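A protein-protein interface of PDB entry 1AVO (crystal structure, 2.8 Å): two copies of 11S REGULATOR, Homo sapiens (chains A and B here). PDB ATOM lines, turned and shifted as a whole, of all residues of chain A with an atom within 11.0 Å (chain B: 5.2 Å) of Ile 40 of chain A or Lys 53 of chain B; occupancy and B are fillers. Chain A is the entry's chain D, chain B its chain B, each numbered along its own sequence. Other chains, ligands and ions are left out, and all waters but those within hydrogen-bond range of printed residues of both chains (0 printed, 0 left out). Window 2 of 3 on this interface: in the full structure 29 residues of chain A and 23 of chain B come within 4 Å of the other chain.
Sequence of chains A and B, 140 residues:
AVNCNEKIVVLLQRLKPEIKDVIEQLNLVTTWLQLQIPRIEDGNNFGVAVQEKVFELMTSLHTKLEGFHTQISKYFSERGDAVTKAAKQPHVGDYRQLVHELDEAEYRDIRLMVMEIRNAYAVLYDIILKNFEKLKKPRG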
ATOM      1  N   GLN A  34     -23.816  20.767   7.476  1.00  0.00           N
ATOM      2  CA  GLN A  34     -23.627  21.528   8.694  1.00  0.00           C
ATOM      3  C   GLN A  34     -24.740  21.205   9.656  1.00  0.00           C
ATOM      4  O   GLN A  34     -24.487  21.017  10.799  1.00  0.00           O
ATOM      5  CB  GLN A  34     -23.649  23.007   8.431  1.00  0.00           C
ATOM      6  CG  GLN A  34     -22.929  23.407   7.184  1.00  0.00           C
ATOM      7  CD  GLN A  34     -22.696  24.895   7.122  1.00  0.00           C
ATOM      8  OE1 GLN A  34     -23.064  25.580   6.142  1.00  0.00           O
ATOM      9  NE2 GLN A  34     -22.069  25.417   8.170  1.00  0.00           N
ATOM     10  N   LEU A  35     -25.988  21.119   9.221  1.00  0.00           N
ATOM     11  CA  LEU A  35     -27.048  20.817  10.160  1.00  0.00           C
ATOM     12  C   LEU A  35     -26.855  19.461  10.844  1.00  0.00           C
ATOM     13  O   LEU A  35     -27.527  19.158  11.796  1.00  0.00           O
ATOM     14  CB  LEU A  35     -28.399  20.863   9.466  1.00  0.00           C
ATOM     15  CG  LEU A  35     -28.782  22.277   9.052  1.00  0.00           C
ATOM     16  CD1 LEU A  35     -30.164  22.317   8.421  1.00  0.00           C
ATOM     17  CD2 LEU A  35     -28.792  23.132  10.237  1.00  0.00           C
ATOM     18  N   GLN A  36     -25.930  18.650  10.351  1.00  0.00           N
ATOM     19  CA  GLN A  36     -25.657  17.305  10.863  1.00  0.00           C
ATOM     20  C   GLN A  36     -24.648  17.348  11.988  1.00  0.00           C
ATOM     21  O   GLN A  36     -24.425  16.362  12.669  1.00  0.00           O
ATOM     22  CB  GLN A  36     -25.039  16.453   9.738  1.00  0.00           C
ATOM     23  CG  GLN A  36     -25.904  15.428   9.043  1.00  0.00           C
ATOM     24  CD  GLN A  36     -27.340  15.637   9.324  1.00  0.00           C
ATOM     25  OE1 GLN A  36     -27.937  14.899  10.113  1.00  0.00           O
ATOM     26  NE2 GLN A  36     -27.908  16.670   8.736  1.00  0.00           N
ATOM     27  N   ILE A  37     -24.009  18.492  12.147  1.00  0.00           N
ATOM     28  CA  ILE A  37     -22.981  18.631  13.147  1.00  0.00           C
ATOM     29  C   ILE A  37     -23.603  18.573  14.510  1.00  0.00           C
ATOM     30  O   ILE A  37     -24.479  19.351  14.818  1.00  0.00           O
ATOM     31  CB  ILE A  37     -22.169  19.900  12.920  1.00  0.00           C
ATOM     32  CG1 ILE A  37     -21.610  19.929  11.486  1.00  0.00           C
ATOM     33  CG2 ILE A  37     -21.042  19.915  13.842  1.00  0.00           C
ATOM     34  CD1 ILE A  37     -20.630  20.999  11.232  1.00  0.00           C
ATOM     35  N   PRO A  38     -23.140  17.653  15.356  1.00  0.00           N
ATOM     36  CA  PRO A  38     -23.643  17.450  16.703  1.00  0.00           C
ATOM     37  C   PRO A  38     -23.140  18.427  17.750  1.00  0.00           C
ATOM     38  O   PRO A  38     -22.122  19.099  17.553  1.00  0.00           O
ATOM     39  CB  PRO A  38     -23.178  16.015  17.002  1.00  0.00           C
ATOM     40  CG  PRO A  38     -21.795  15.962  16.397  1.00  0.00           C
ATOM     41  CD  PRO A  38     -21.988  16.757  15.090  1.00  0.00           C
ATOM     42  N   ARG A  39     -23.848  18.455  18.878  1.00  0.00           N
ATOM     43  CA  ARG A  39     -23.505  19.288  20.009  1.00  0.00           C
ATOM     44  C   ARG A  39     -22.045  19.080  20.335  1.00  0.00           C
ATOM     45  O   ARG A  39     -21.594  17.938  20.416  1.00  0.00           O
ATOM     46  CB  ARG A  39     -24.329  18.883  21.215  1.00  0.00           C
ATOM     47  CG  ARG A  39     -24.266  19.918  22.272  1.00  0.00           C
ATOM     48  CD  ARG A  39     -24.649  19.413  23.641  1.00  0.00           C
ATOM     49  NE  ARG A  39     -25.745  18.467  23.562  1.00  0.00           N
ATOM     50  CZ  ARG A  39     -25.766  17.355  24.319  1.00  0.00           C
ATOM     51  NH1 ARG A  39     -24.756  17.094  25.222  1.00  0.00           N
ATOM     52  NH2 ARG A  39     -26.667  16.378  24.067  1.00  0.00           N
ATOM     53  N   ILE A  40     -21.311  20.170  20.544  1.00  0.00           N
ATOM     54  CA  ILE A  40     -19.876  20.079  20.826  1.00  0.00           C
ATOM     55  C   ILE A  40     -19.774  19.426  22.154  1.00  0.00           C
ATOM     56  O   ILE A  40     -20.343  19.912  23.132  1.00  0.00           O
ATOM     57  CB  ILE A  40     -19.240  21.434  20.917  1.00  0.00           C
ATOM     58  CG1 ILE A  40     -19.535  22.210  19.662  1.00  0.00           C
ATOM     59  CG2 ILE A  40     -17.817  21.306  21.144  1.00  0.00           C
ATOM     60  CD1 ILE A  40     -18.802  23.440  19.486  1.00  0.00           C
ATOM     61  N   GLU A  41     -19.114  18.275  22.159  1.00  0.00           N
ATOM     62  CA  GLU A  41     -18.923  17.465  23.362  1.00  0.00           C
ATOM     63  C   GLU A  41     -17.469  17.153  23.550  1.00  0.00           C
ATOM     64  O   GLU A  41     -16.687  17.230  22.622  1.00  0.00           O
ATOM     65  CB  GLU A  41     -19.719  16.174  23.291  1.00  0.00           C
ATOM     66  CG  GLU A  41     -21.194  16.398  23.444  1.00  0.00           C
ATOM     67  CD  GLU A  41     -22.012  15.129  23.473  1.00  0.00           C
ATOM     68  OE1 GLU A  41     -21.405  14.039  23.495  1.00  0.00           O
ATOM     69  OE2 GLU A  41     -23.271  15.216  23.462  1.00  0.00           O
ATOM     70  N   ASP A  42     -17.109  16.809  24.777  1.00  0.00           N
ATOM     71  CA  ASP A  42     -15.732  16.520  25.123  1.00  0.00           C
ATOM     72  C   ASP A  42     -15.076  15.294  24.455  1.00  0.00           C
ATOM     73  O   ASP A  42     -13.899  15.332  24.060  1.00  0.00           O
ATOM     74  CB  ASP A  42     -15.635  16.434  26.626  1.00  0.00           C
ATOM     75  CG  ASP A  42     -14.268  16.805  27.127  1.00  0.00           C
ATOM     76  OD1 ASP A  42     -13.423  17.229  26.300  1.00  0.00           O
ATOM     77  OD2 ASP A  42     -14.030  16.669  28.351  1.00  0.00           O
ATOM     78  N   GLY A  43     -15.807  14.193  24.337  1.00  0.00           N
ATOM     79  CA  GLY A  43     -15.211  13.045  23.691  1.00  0.00           C
ATOM     80  C   GLY A  43     -16.102  12.493  22.602  1.00  0.00           C
ATOM     81  O   GLY A  43     -17.266  12.886  22.479  1.00  0.00           O
ATOM     82  N   ASN A  44     -15.531  11.587  21.812  1.00  0.00           N
ATOM     83  CA  ASN A  44     -16.215  10.915  20.726  1.00  0.00           C
ATOM     84  C   ASN A  44     -16.389  11.889  19.591  1.00  0.00           C
ATOM     85  O   ASN A  44     -17.518  12.264  19.272  1.00  0.00           O
ATOM     86  CB  ASN A  44     -17.565  10.395  21.226  1.00  0.00           C
ATOM     87  CG  ASN A  44     -18.233   9.441  20.264  1.00  0.00           C
ATOM     88  OD1 ASN A  44     -17.608   8.906  19.342  1.00  0.00           O
ATOM     89  ND2 ASN A  44     -19.518   9.198  20.493  1.00  0.00           N
ATOM     90  N   ASN A  45     -15.280  12.291  18.971  1.00  0.00           N
ATOM     91  CA  ASN A  45     -15.381  13.251  17.885  1.00  0.00           C
ATOM     92  C   ASN A  45     -14.824  12.808  16.550  1.00  0.00           C
ATOM     93  O   ASN A  45     -14.617  13.631  15.620  1.00  0.00           O
ATOM     94  CB  ASN A  45     -14.751  14.573  18.282  1.00  0.00           C
ATOM     95  CG  ASN A  45     -15.337  15.139  19.553  1.00  0.00           C
ATOM     96  OD1 ASN A  45     -16.553  15.336  19.670  1.00  0.00           O
ATOM     97  ND2 ASN A  45     -14.462  15.434  20.514  1.00  0.00           N
ATOM     98  N   PHE A  46     -14.659  11.495  16.414  1.00  0.00           N
ATOM     99  CA  PHE A  46     -14.140  10.972  15.169  1.00  0.00           C
ATOM    100  C   PHE A  46     -15.095  11.316  14.084  1.00  0.00           C
ATOM    101  O   PHE A  46     -14.692  11.872  13.103  1.00  0.00           O
ATOM    102  CB  PHE A  46     -13.977   9.471  15.193  1.00  0.00           C
ATOM    103  CG  PHE A  46     -13.436   8.920  13.905  1.00  0.00           C
ATOM    104  CD1 PHE A  46     -12.248   9.397  13.386  1.00  0.00           C
ATOM    105  CD2 PHE A  46     -14.166   7.999  13.173  1.00  0.00           C
ATOM    106  CE1 PHE A  46     -11.811   8.989  12.167  1.00  0.00           C
ATOM    107  CE2 PHE A  46     -13.732   7.571  11.925  1.00  0.00           C
ATOM    108  CZ  PHE A  46     -12.558   8.069  11.421  1.00  0.00           C
ATOM    109  N   GLY A  47     -16.365  10.993  14.300  1.00  0.00           N
ATOM    110  CA  GLY A  47     -17.403  11.279  13.332  1.00  0.00           C
ATOM    111  C   GLY A  47     -17.416  12.750  13.045  1.00  0.00           C
ATOM    112  O   GLY A  47     -17.567  13.154  11.892  1.00  0.00           O
ATOM    113  N   VAL A  48     -17.210  13.547  14.087  1.00  0.00           N
ATOM    114  CA  VAL A  48     -17.178  14.967  13.890  1.00  0.00           C
ATOM    115  C   VAL A  48     -15.983  15.318  12.966  1.00  0.00           C
ATOM    116  O   VAL A  48     -16.063  16.173  12.055  1.00  0.00           O
ATOM    117  CB  VAL A  48     -17.067  15.642  15.211  1.00  0.00           C
ATOM    118  CG1 VAL A  48     -16.771  17.042  14.993  1.00  0.00           C
ATOM    119  CG2 VAL A  48     -18.382  15.498  15.992  1.00  0.00           C
ATOM    120  N   ALA A  49     -14.874  14.616  13.184  1.00  0.00           N
ATOM    121  CA  ALA A  49     -13.680  14.821  12.372  1.00  0.00           C
ATOM    122  C   ALA A  49     -13.948  14.482  10.903  1.00  0.00           C
ATOM    123  O   ALA A  49     -13.416  15.098   9.985  1.00  0.00           O
ATOM    124  CB  ALA A  49     -12.616  13.955  12.886  1.00  0.00           C
ATOM    125  N   GLN A  51     -16.901  14.651   9.396  1.00  0.00           N
ATOM    126  CA  GLN A  51     -17.722  15.658   8.770  1.00  0.00           C
ATOM    127  C   GLN A  51     -16.844  16.829   8.385  1.00  0.00           C
ATOM    128  O   GLN A  51     -17.027  17.411   7.307  1.00  0.00           O
ATOM    129  CB  GLN A  51     -18.826  16.144   9.708  1.00  0.00           C
ATOM    130  CG  GLN A  51     -19.745  15.065  10.264  1.00  0.00           C
ATOM    131  CD  GLN A  51     -20.771  15.605  11.226  1.00  0.00           C
ATOM    132  OE1 GLN A  51     -20.532  16.602  11.894  1.00  0.00           O
ATOM    133  NE2 GLN A  51     -21.923  14.957  11.309  1.00  0.00           N
ATOM    134  N   GLU A  52     -15.879  17.166   9.237  1.00  0.00           N
ATOM    135  CA  GLU A  52     -15.005  18.305   8.947  1.00  0.00           C
ATOM    136  C   GLU A  52     -14.146  18.120   7.717  1.00  0.00           C
ATOM    137  O   GLU A  52     -13.827  19.076   7.043  1.00  0.00           O
ATOM    138  CB  GLU A  52     -14.110  18.624  10.126  1.00  0.00           C
ATOM    139  CG  GLU A  52     -14.856  18.985  11.401  1.00  0.00           C
ATOM    140  CD  GLU A  52     -13.913  19.316  12.591  1.00  0.00           C
ATOM    141  OE1 GLU A  52     -12.712  18.897  12.584  1.00  0.00           O
ATOM    142  OE2 GLU A  52     -14.379  19.986  13.555  1.00  0.00           O
ATOM    143  N   LYS A  53     -13.755  16.894   7.423  1.00  0.00           N
ATOM    144  CA  LYS A  53     -12.937  16.644   6.243  1.00  0.00           C
ATOM    145  C   LYS A  53     -13.722  16.711   4.952  1.00  0.00           C
ATOM    146  O   LYS A  53     -13.188  17.070   3.912  1.00  0.00           O
ATOM    147  CB  LYS A  53     -12.293  15.275   6.353  1.00  0.00           C
ATOM    148  CG  LYS A  53     -11.564  14.860   5.126  1.00  0.00           C
ATOM    149  CD  LYS A  53     -10.097  15.219   5.181  1.00  0.00           C
ATOM    150  CE  LYS A  53      -9.493  15.200   3.785  1.00  0.00           C
ATOM    151  NZ  LYS A  53      -8.230  15.992   3.699  1.00  0.00           N
ATOM    152  N   PHE A  55     -16.466  18.406   4.625  1.00  0.00           N
ATOM    153  CA  PHE A  55     -16.761  19.791   4.558  1.00  0.00           C
ATOM    154  C   PHE A  55     -15.676  20.524   3.864  1.00  0.00           C
ATOM    155  O   PHE A  55     -15.933  21.358   3.008  1.00  0.00           O
ATOM    156  CB  PHE A  55     -16.862  20.320   5.914  1.00  0.00           C
ATOM    157  CG  PHE A  55     -17.833  21.368   6.010  1.00  0.00           C
ATOM    158  CD1 PHE A  55     -19.172  21.062   6.189  1.00  0.00           C
ATOM    159  CD2 PHE A  55     -17.440  22.678   5.780  1.00  0.00           C
ATOM    160  CE1 PHE A  55     -20.117  22.052   6.126  1.00  0.00           C
ATOM    161  CE2 PHE A  55     -18.358  23.710   5.712  1.00  0.00           C
ATOM    162  CZ  PHE A  55     -19.705  23.401   5.878  1.00  0.00           C
ATOM    163  N   GLU A  56     -14.440  20.208   4.198  1.00  0.00           N
ATOM    164  CA  GLU A  56     -13.314  20.862   3.519  1.00  0.00           C
ATOM    165  C   GLU A  56     -13.432  20.689   2.040  1.00  0.00           C
ATOM    166  O   GLU A  56     -13.145  21.572   1.298  1.00  0.00           O
ATOM    167  CB  GLU A  56     -11.988  20.232   3.885  1.00  0.00           C
ATOM    168  CG  GLU A  56     -11.421  20.626   5.248  1.00  0.00           C
ATOM    169  CD  GLU A  56     -10.138  19.842   5.597  1.00  0.00           C
ATOM    170  OE1 GLU A  56      -9.400  19.406   4.659  1.00  0.00           O
ATOM    171  OE2 GLU A  56      -9.869  19.658   6.819  1.00  0.00           O
ATOM    172  N   PRO A 138     -22.568  10.810  13.415  1.00  0.00           N
ATOM    173  CA  PRO A 138     -21.216  10.938  13.899  1.00  0.00           C
ATOM    174  C   PRO A 138     -20.918  10.294  15.191  1.00  0.00           C
ATOM    175  O   PRO A 138     -19.743  10.110  15.510  1.00  0.00           O
ATOM    176  CB  PRO A 138     -21.039  12.439  14.000  1.00  0.00           C
ATOM    177  CG  PRO A 138     -22.339  12.929  14.245  1.00  0.00           C
ATOM    178  CD  PRO A 138     -23.186  12.139  13.315  1.00  0.00           C
ATOM    179  N   ARG A 139     -21.945   9.970  15.961  1.00  0.00           N
ATOM    180  CA  ARG A 139     -21.714   9.347  17.272  1.00  0.00           C
ATOM    181  C   ARG A 139     -22.328   7.969  17.479  1.00  0.00           C
ATOM    182  O   ARG A 139     -21.899   7.239  18.378  1.00  0.00           O
ATOM    183  CB  ARG A 139     -22.082  10.306  18.420  1.00  0.00           C
ATOM    184  CG  ARG A 139     -21.049  11.417  18.595  1.00  0.00           C
ATOM    185  CD  ARG A 139     -21.412  12.515  19.553  1.00  0.00           C
ATOM    186  NE  ARG A 139     -20.319  13.477  19.633  1.00  0.00           N
ATOM    187  CZ  ARG A 139     -20.492  14.745  19.952  1.00  0.00           C
ATOM    188  NH1 ARG A 139     -21.722  15.183  20.252  1.00  0.00           N
ATOM    189  NH2 ARG A 139     -19.481  15.603  19.818  1.00  0.00           N
ATOM    190  N   PHE B  46     -13.931  24.096  28.743  1.00  0.00           N
ATOM    191  CA  PHE B  46     -14.561  23.376  27.677  1.00  0.00           C
ATOM    192  C   PHE B  46     -15.633  24.260  27.126  1.00  0.00           C
ATOM    193  O   PHE B  46     -15.680  24.503  25.931  1.00  0.00           O
ATOM    194  CB  PHE B  46     -15.164  22.070  28.147  1.00  0.00           C
ATOM    195  CG  PHE B  46     -15.863  21.343  27.053  1.00  0.00           C
ATOM    196  CD1 PHE B  46     -15.165  20.995  25.889  1.00  0.00           C
ATOM    197  CD2 PHE B  46     -17.239  21.092  27.139  1.00  0.00           C
ATOM    198  CE1 PHE B  46     -15.812  20.425  24.837  1.00  0.00           C
ATOM    199  CE2 PHE B  46     -17.915  20.516  26.082  1.00  0.00           C
ATOM    200  CZ  PHE B  46     -17.202  20.180  24.923  1.00  0.00           C
ATOM    201  N   ALA B  49     -14.393  26.795  25.152  1.00  0.00           N
ATOM    202  CA  ALA B  49     -14.027  26.229  23.857  1.00  0.00           C
ATOM    203  C   ALA B  49     -15.259  26.111  22.941  1.00  0.00           C
ATOM    204  O   ALA B  49     -15.185  26.312  21.730  1.00  0.00           O
ATOM    205  CB  ALA B  49     -13.419  24.890  24.059  1.00  0.00           C
ATOM    206  N   VAL B  50     -16.390  25.765  23.524  1.00  0.00           N
ATOM    207  CA  VAL B  50     -17.622  25.656  22.769  1.00  0.00           C
ATOM    208  C   VAL B  50     -18.057  27.031  22.267  1.00  0.00           C
ATOM    209  O   VAL B  50     -18.528  27.139  21.163  1.00  0.00           O
ATOM    210  CB  VAL B  50     -18.727  25.155  23.658  1.00  0.00           C
ATOM    211  CG1 VAL B  50     -20.033  25.338  22.980  1.00  0.00           C
ATOM    212  CG2 VAL B  50     -18.488  23.732  24.038  1.00  0.00           C
ATOM    213  N   GLN B  51     -17.928  28.067  23.085  1.00  0.00           N
ATOM    214  CA  GLN B  51     -18.327  29.381  22.663  1.00  0.00           C
ATOM    215  C   GLN B  51     -17.444  29.843  21.542  1.00  0.00           C
ATOM    216  O   GLN B  51     -17.931  30.508  20.612  1.00  0.00           O
ATOM    217  CB  GLN B  51     -18.202  30.374  23.791  1.00  0.00           C
ATOM    218  CG  GLN B  51     -19.002  30.050  25.049  1.00  0.00           C
ATOM    219  CD  GLN B  51     -18.803  31.074  26.130  1.00  0.00           C
ATOM    220  OE1 GLN B  51     -17.773  31.738  26.161  1.00  0.00           O
ATOM    221  NE2 GLN B  51     -19.779  31.223  27.020  1.00  0.00           N
ATOM    222  N   GLU B  52     -16.162  29.469  21.600  1.00  0.00           N
ATOM    223  CA  GLU B  52     -15.221  29.866  20.548  1.00  0.00           C
ATOM    224  C   GLU B  52     -15.514  29.240  19.197  1.00  0.00           C
ATOM    225  O   GLU B  52     -15.258  29.850  18.173  1.00  0.00           O
ATOM    226  CB  GLU B  52     -13.788  29.548  20.931  1.00  0.00           C
ATOM    227  CG  GLU B  52     -13.302  30.253  22.189  1.00  0.00           C
ATOM    228  CD  GLU B  52     -11.824  29.926  22.569  1.00  0.00           C
ATOM    229  OE1 GLU B  52     -11.279  28.857  22.168  1.00  0.00           O
ATOM    230  OE2 GLU B  52     -11.194  30.733  23.297  1.00  0.00           O
ATOM    231  N   LYS B  53     -16.013  28.012  19.192  1.00  0.00           N
ATOM    232  CA  LYS B  53     -16.321  27.334  17.951  1.00  0.00           C
ATOM    233  C   LYS B  53     -17.573  27.876  17.258  1.00  0.00           C
ATOM    234  O   LYS B  53     -17.663  27.852  16.016  1.00  0.00           O
ATOM    235  CB  LYS B  53     -16.460  25.846  18.215  1.00  0.00           C
ATOM    236  CG  LYS B  53     -16.922  25.070  17.034  1.00  0.00           C
ATOM    237  CD  LYS B  53     -15.796  24.516  16.208  1.00  0.00           C
ATOM    238  CE  LYS B  53     -16.299  24.174  14.821  1.00  0.00           C
ATOM    239  NZ  LYS B  53     -15.164  23.993  13.871  1.00  0.00           N
ATOM    240  N   VAL B  54     -18.578  28.247  18.065  1.00  0.00           N
ATOM    241  CA  VAL B  54     -19.823  28.810  17.544  1.00  0.00           C
ATOM    242  C   VAL B  54     -19.480  30.166  16.988  1.00  0.00           C
ATOM    243  O   VAL B  54     -19.901  30.594  15.922  1.00  0.00           O
ATOM    244  CB  VAL B  54     -20.816  29.008  18.641  1.00  0.00           C
ATOM    245  CG1 VAL B  54     -22.039  29.705  18.110  1.00  0.00           C
ATOM    246  CG2 VAL B  54     -21.202  27.681  19.178  1.00  0.00           C
ATOM    247  N   PHE B  55     -18.666  30.842  17.747  1.00  0.00           N
ATOM    248  CA  PHE B  55     -18.224  32.139  17.342  1.00  0.00           C
ATOM    249  C   PHE B  55     -17.572  32.100  15.995  1.00  0.00           C
ATOM    250  O   PHE B  55     -17.782  32.980  15.160  1.00  0.00           O
ATOM    251  CB  PHE B  55     -17.232  32.637  18.314  1.00  0.00           C
ATOM    252  CG  PHE B  55     -17.300  34.068  18.469  1.00  0.00           C
ATOM    253  CD1 PHE B  55     -18.234  34.623  19.319  1.00  0.00           C
ATOM    254  CD2 PHE B  55     -16.502  34.886  17.670  1.00  0.00           C
ATOM    255  CE1 PHE B  55     -18.383  35.973  19.370  1.00  0.00           C
ATOM    256  CE2 PHE B  55     -16.620  36.264  17.695  1.00  0.00           C
ATOM    257  CZ  PHE B  55     -17.564  36.812  18.540  1.00  0.00           C
ATOM    258  N   GLU B  56     -16.759  31.090  15.770  1.00  0.00           N
ATOM    259  CA  GLU B  56     -16.119  30.981  14.476  1.00  0.00           C
ATOM    260  C   GLU B  56     -17.160  30.968  13.389  1.00  0.00           C
ATOM    261  O   GLU B  56     -16.974  31.532  12.351  1.00  0.00           O
ATOM    262  CB  GLU B  56     -15.365  29.669  14.361  1.00  0.00           C
ATOM    263  CG  GLU B  56     -13.990  29.626  15.015  1.00  0.00           C
ATOM    264  CD  GLU B  56     -13.357  28.232  14.925  1.00  0.00           C
ATOM    265  OE1 GLU B  56     -13.693  27.480  13.968  1.00  0.00           O
ATOM    266  OE2 GLU B  56     -12.534  27.888  15.818  1.00  0.00           O
ATOM    267  N   LEU B  57     -18.254  30.273  13.624  1.00  0.00           N
ATOM    268  CA  LEU B  57     -19.263  30.195  12.606  1.00  0.00           C
ATOM    269  C   LEU B  57     -19.916  31.522  12.350  1.00  0.00           C
ATOM    270  O   LEU B  57     -20.058  31.923  11.218  1.00  0.00           O
ATOM    271  CB  LEU B  57     -20.298  29.174  12.989  1.00  0.00           C
ATOM    272  CG  LEU B  57     -21.528  29.310  12.110  1.00  0.00           C
ATOM    273  CD1 LEU B  57     -21.507  28.343  10.997  1.00  0.00           C
ATOM    274  CD2 LEU B  57     -22.722  29.053  12.918  1.00  0.00           C
ATOM    275  N   ILE B 127     -27.133  25.590  15.450  1.00  0.00           N
ATOM    276  CA  ILE B 127     -25.977  25.564  16.326  1.00  0.00           C
ATOM    277  C   ILE B 127     -26.141  26.232  17.680  1.00  0.00           C
ATOM    278  O   ILE B 127     -25.552  25.782  18.639  1.00  0.00           O
ATOM    279  CB  ILE B 127     -24.746  26.154  15.638  1.00  0.00           C
ATOM    280  CG1 ILE B 127     -23.512  25.765  16.414  1.00  0.00           C
ATOM    281  CG2 ILE B 127     -24.807  27.671  15.591  1.00  0.00           C
ATOM    282  CD1 ILE B 127     -22.231  25.942  15.629  1.00  0.00           C
ATOM    283  N   ASN B 131     -26.004  23.805  21.408  1.00  0.00           N
ATOM    284  CA  ASN B 131     -25.042  24.128  22.443  1.00  0.00           C
ATOM    285  C   ASN B 131     -25.437  25.231  23.349  1.00  0.00           C
ATOM    286  O   ASN B 131     -24.568  25.898  23.870  1.00  0.00           O
ATOM    287  CB  ASN B 131     -23.770  24.573  21.778  1.00  0.00           C
ATOM    288  CG  ASN B 131     -23.318  23.608  20.726  1.00  0.00           C
ATOM    289  OD1 ASN B 131     -22.630  22.606  21.004  1.00  0.00           O
ATOM    290  ND2 ASN B 131     -23.697  23.883  19.524  1.00  0.00           N
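The side-chain amide oxygen of Asn 131 of chain B is in hydrogen-bond range of the backbone NH of Ile 40 of chain A, at 2.8 Å.
OE1 of Glu 56 of chain B lies within salt-bridge range of NZ of Lys 53 of chain B, at 3.8 Å. The guanidinium group of Arg 139 of chain A is in salt-bridge range of the side-chain carboxylate of Glu 41 of chain A, at 3.5 Å. The guanidinium group of Arg 39 of chain A lies within salt-bridge range of the side-chain carboxylate of Glu 41 of chain A (3.0 Å). O of Ile 127 of chain B lies within hydrogen-bond range of ND2 of Asn 131 of chain B (2.8 Å). O of Arg 39 of chain A lies within hydrogen-bond range of NH1 of Arg 139 of chain A, 2.8 Å away.
Asn 131 of chain B touches Arg 39 of chain A (OD1 to CG, 3.4 Å). Ile 40 of chain A touches Phe 46 of chain B (O to CZ, 3.6 Å). Val 50 of chain B touches Ile 40 of chain A (CG2 to CG2, 3.8 Å). CG of Lys 53 of chain B touches CD1 of Ile 40 of chain A, at 3.5 Å. Phe 46 of chain B touches Glu 41 of chain A (CZ to C, 3.3 Å). CZ of Phe 46 of chain B touches N of Asp 42 of chain A, 3.4 Å away.
Of chain B, only Phe 46 (3.6 Å), Val 50 (3.8 Å), Lys 53 (3.5 Å) and Asn 131 (2.8 Å) come within 4 Å of Ile 40 of chain A. Of chain A, only Ile 40 (3.5 Å) comes within 4 Å of Lys 53 of chain B. No residue of chain A comes within 4 Å of Ala 49 of chain B. Val 50 of chain B touches just one residue of chain A: Ile 40. Val 54 of chain B touches none of the printed residues of chain A. Of the printed residues of chain A, Phe 46 of chain B touches Ile 40, Glu 41 and Asp 42. Printed residues of chain B within 4 Å of Glu 41 of chain A: Phe 46. Printed residues of chain B within 4 Å of Arg 39 of chain A: Asn 131. Printed residues of chain B within 4 Å of Asp 42 of chain A: Phe 46 (3.4 Å). The nearest residue of chain B that does not touch Ile 40 of chain A is Val 54 of chain B (4.9 Å). The nearest residue of chain A that does not touch Lys 53 of chain B is Glu 52 of chain A (4.1 Å).
Of the 23 printed residues of chain A, 4 touch a printed residue of chain B. Hydrophobic or aromatic side chains of chain A that line the printed part of chain B: Ile 40. Hydrophobic or aromatic side chains of chain B that line the printed part of chain A: Phe 46 and Val 50. Among the printed residues, 7 pairs touch across the chains.
Positions printed for both chains: 46, 49, 51, 52, 53, 55 and 56. Of the 7 pairs that touch across the chains among the printed residues, none has its exchanged pair printed and touching as well.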
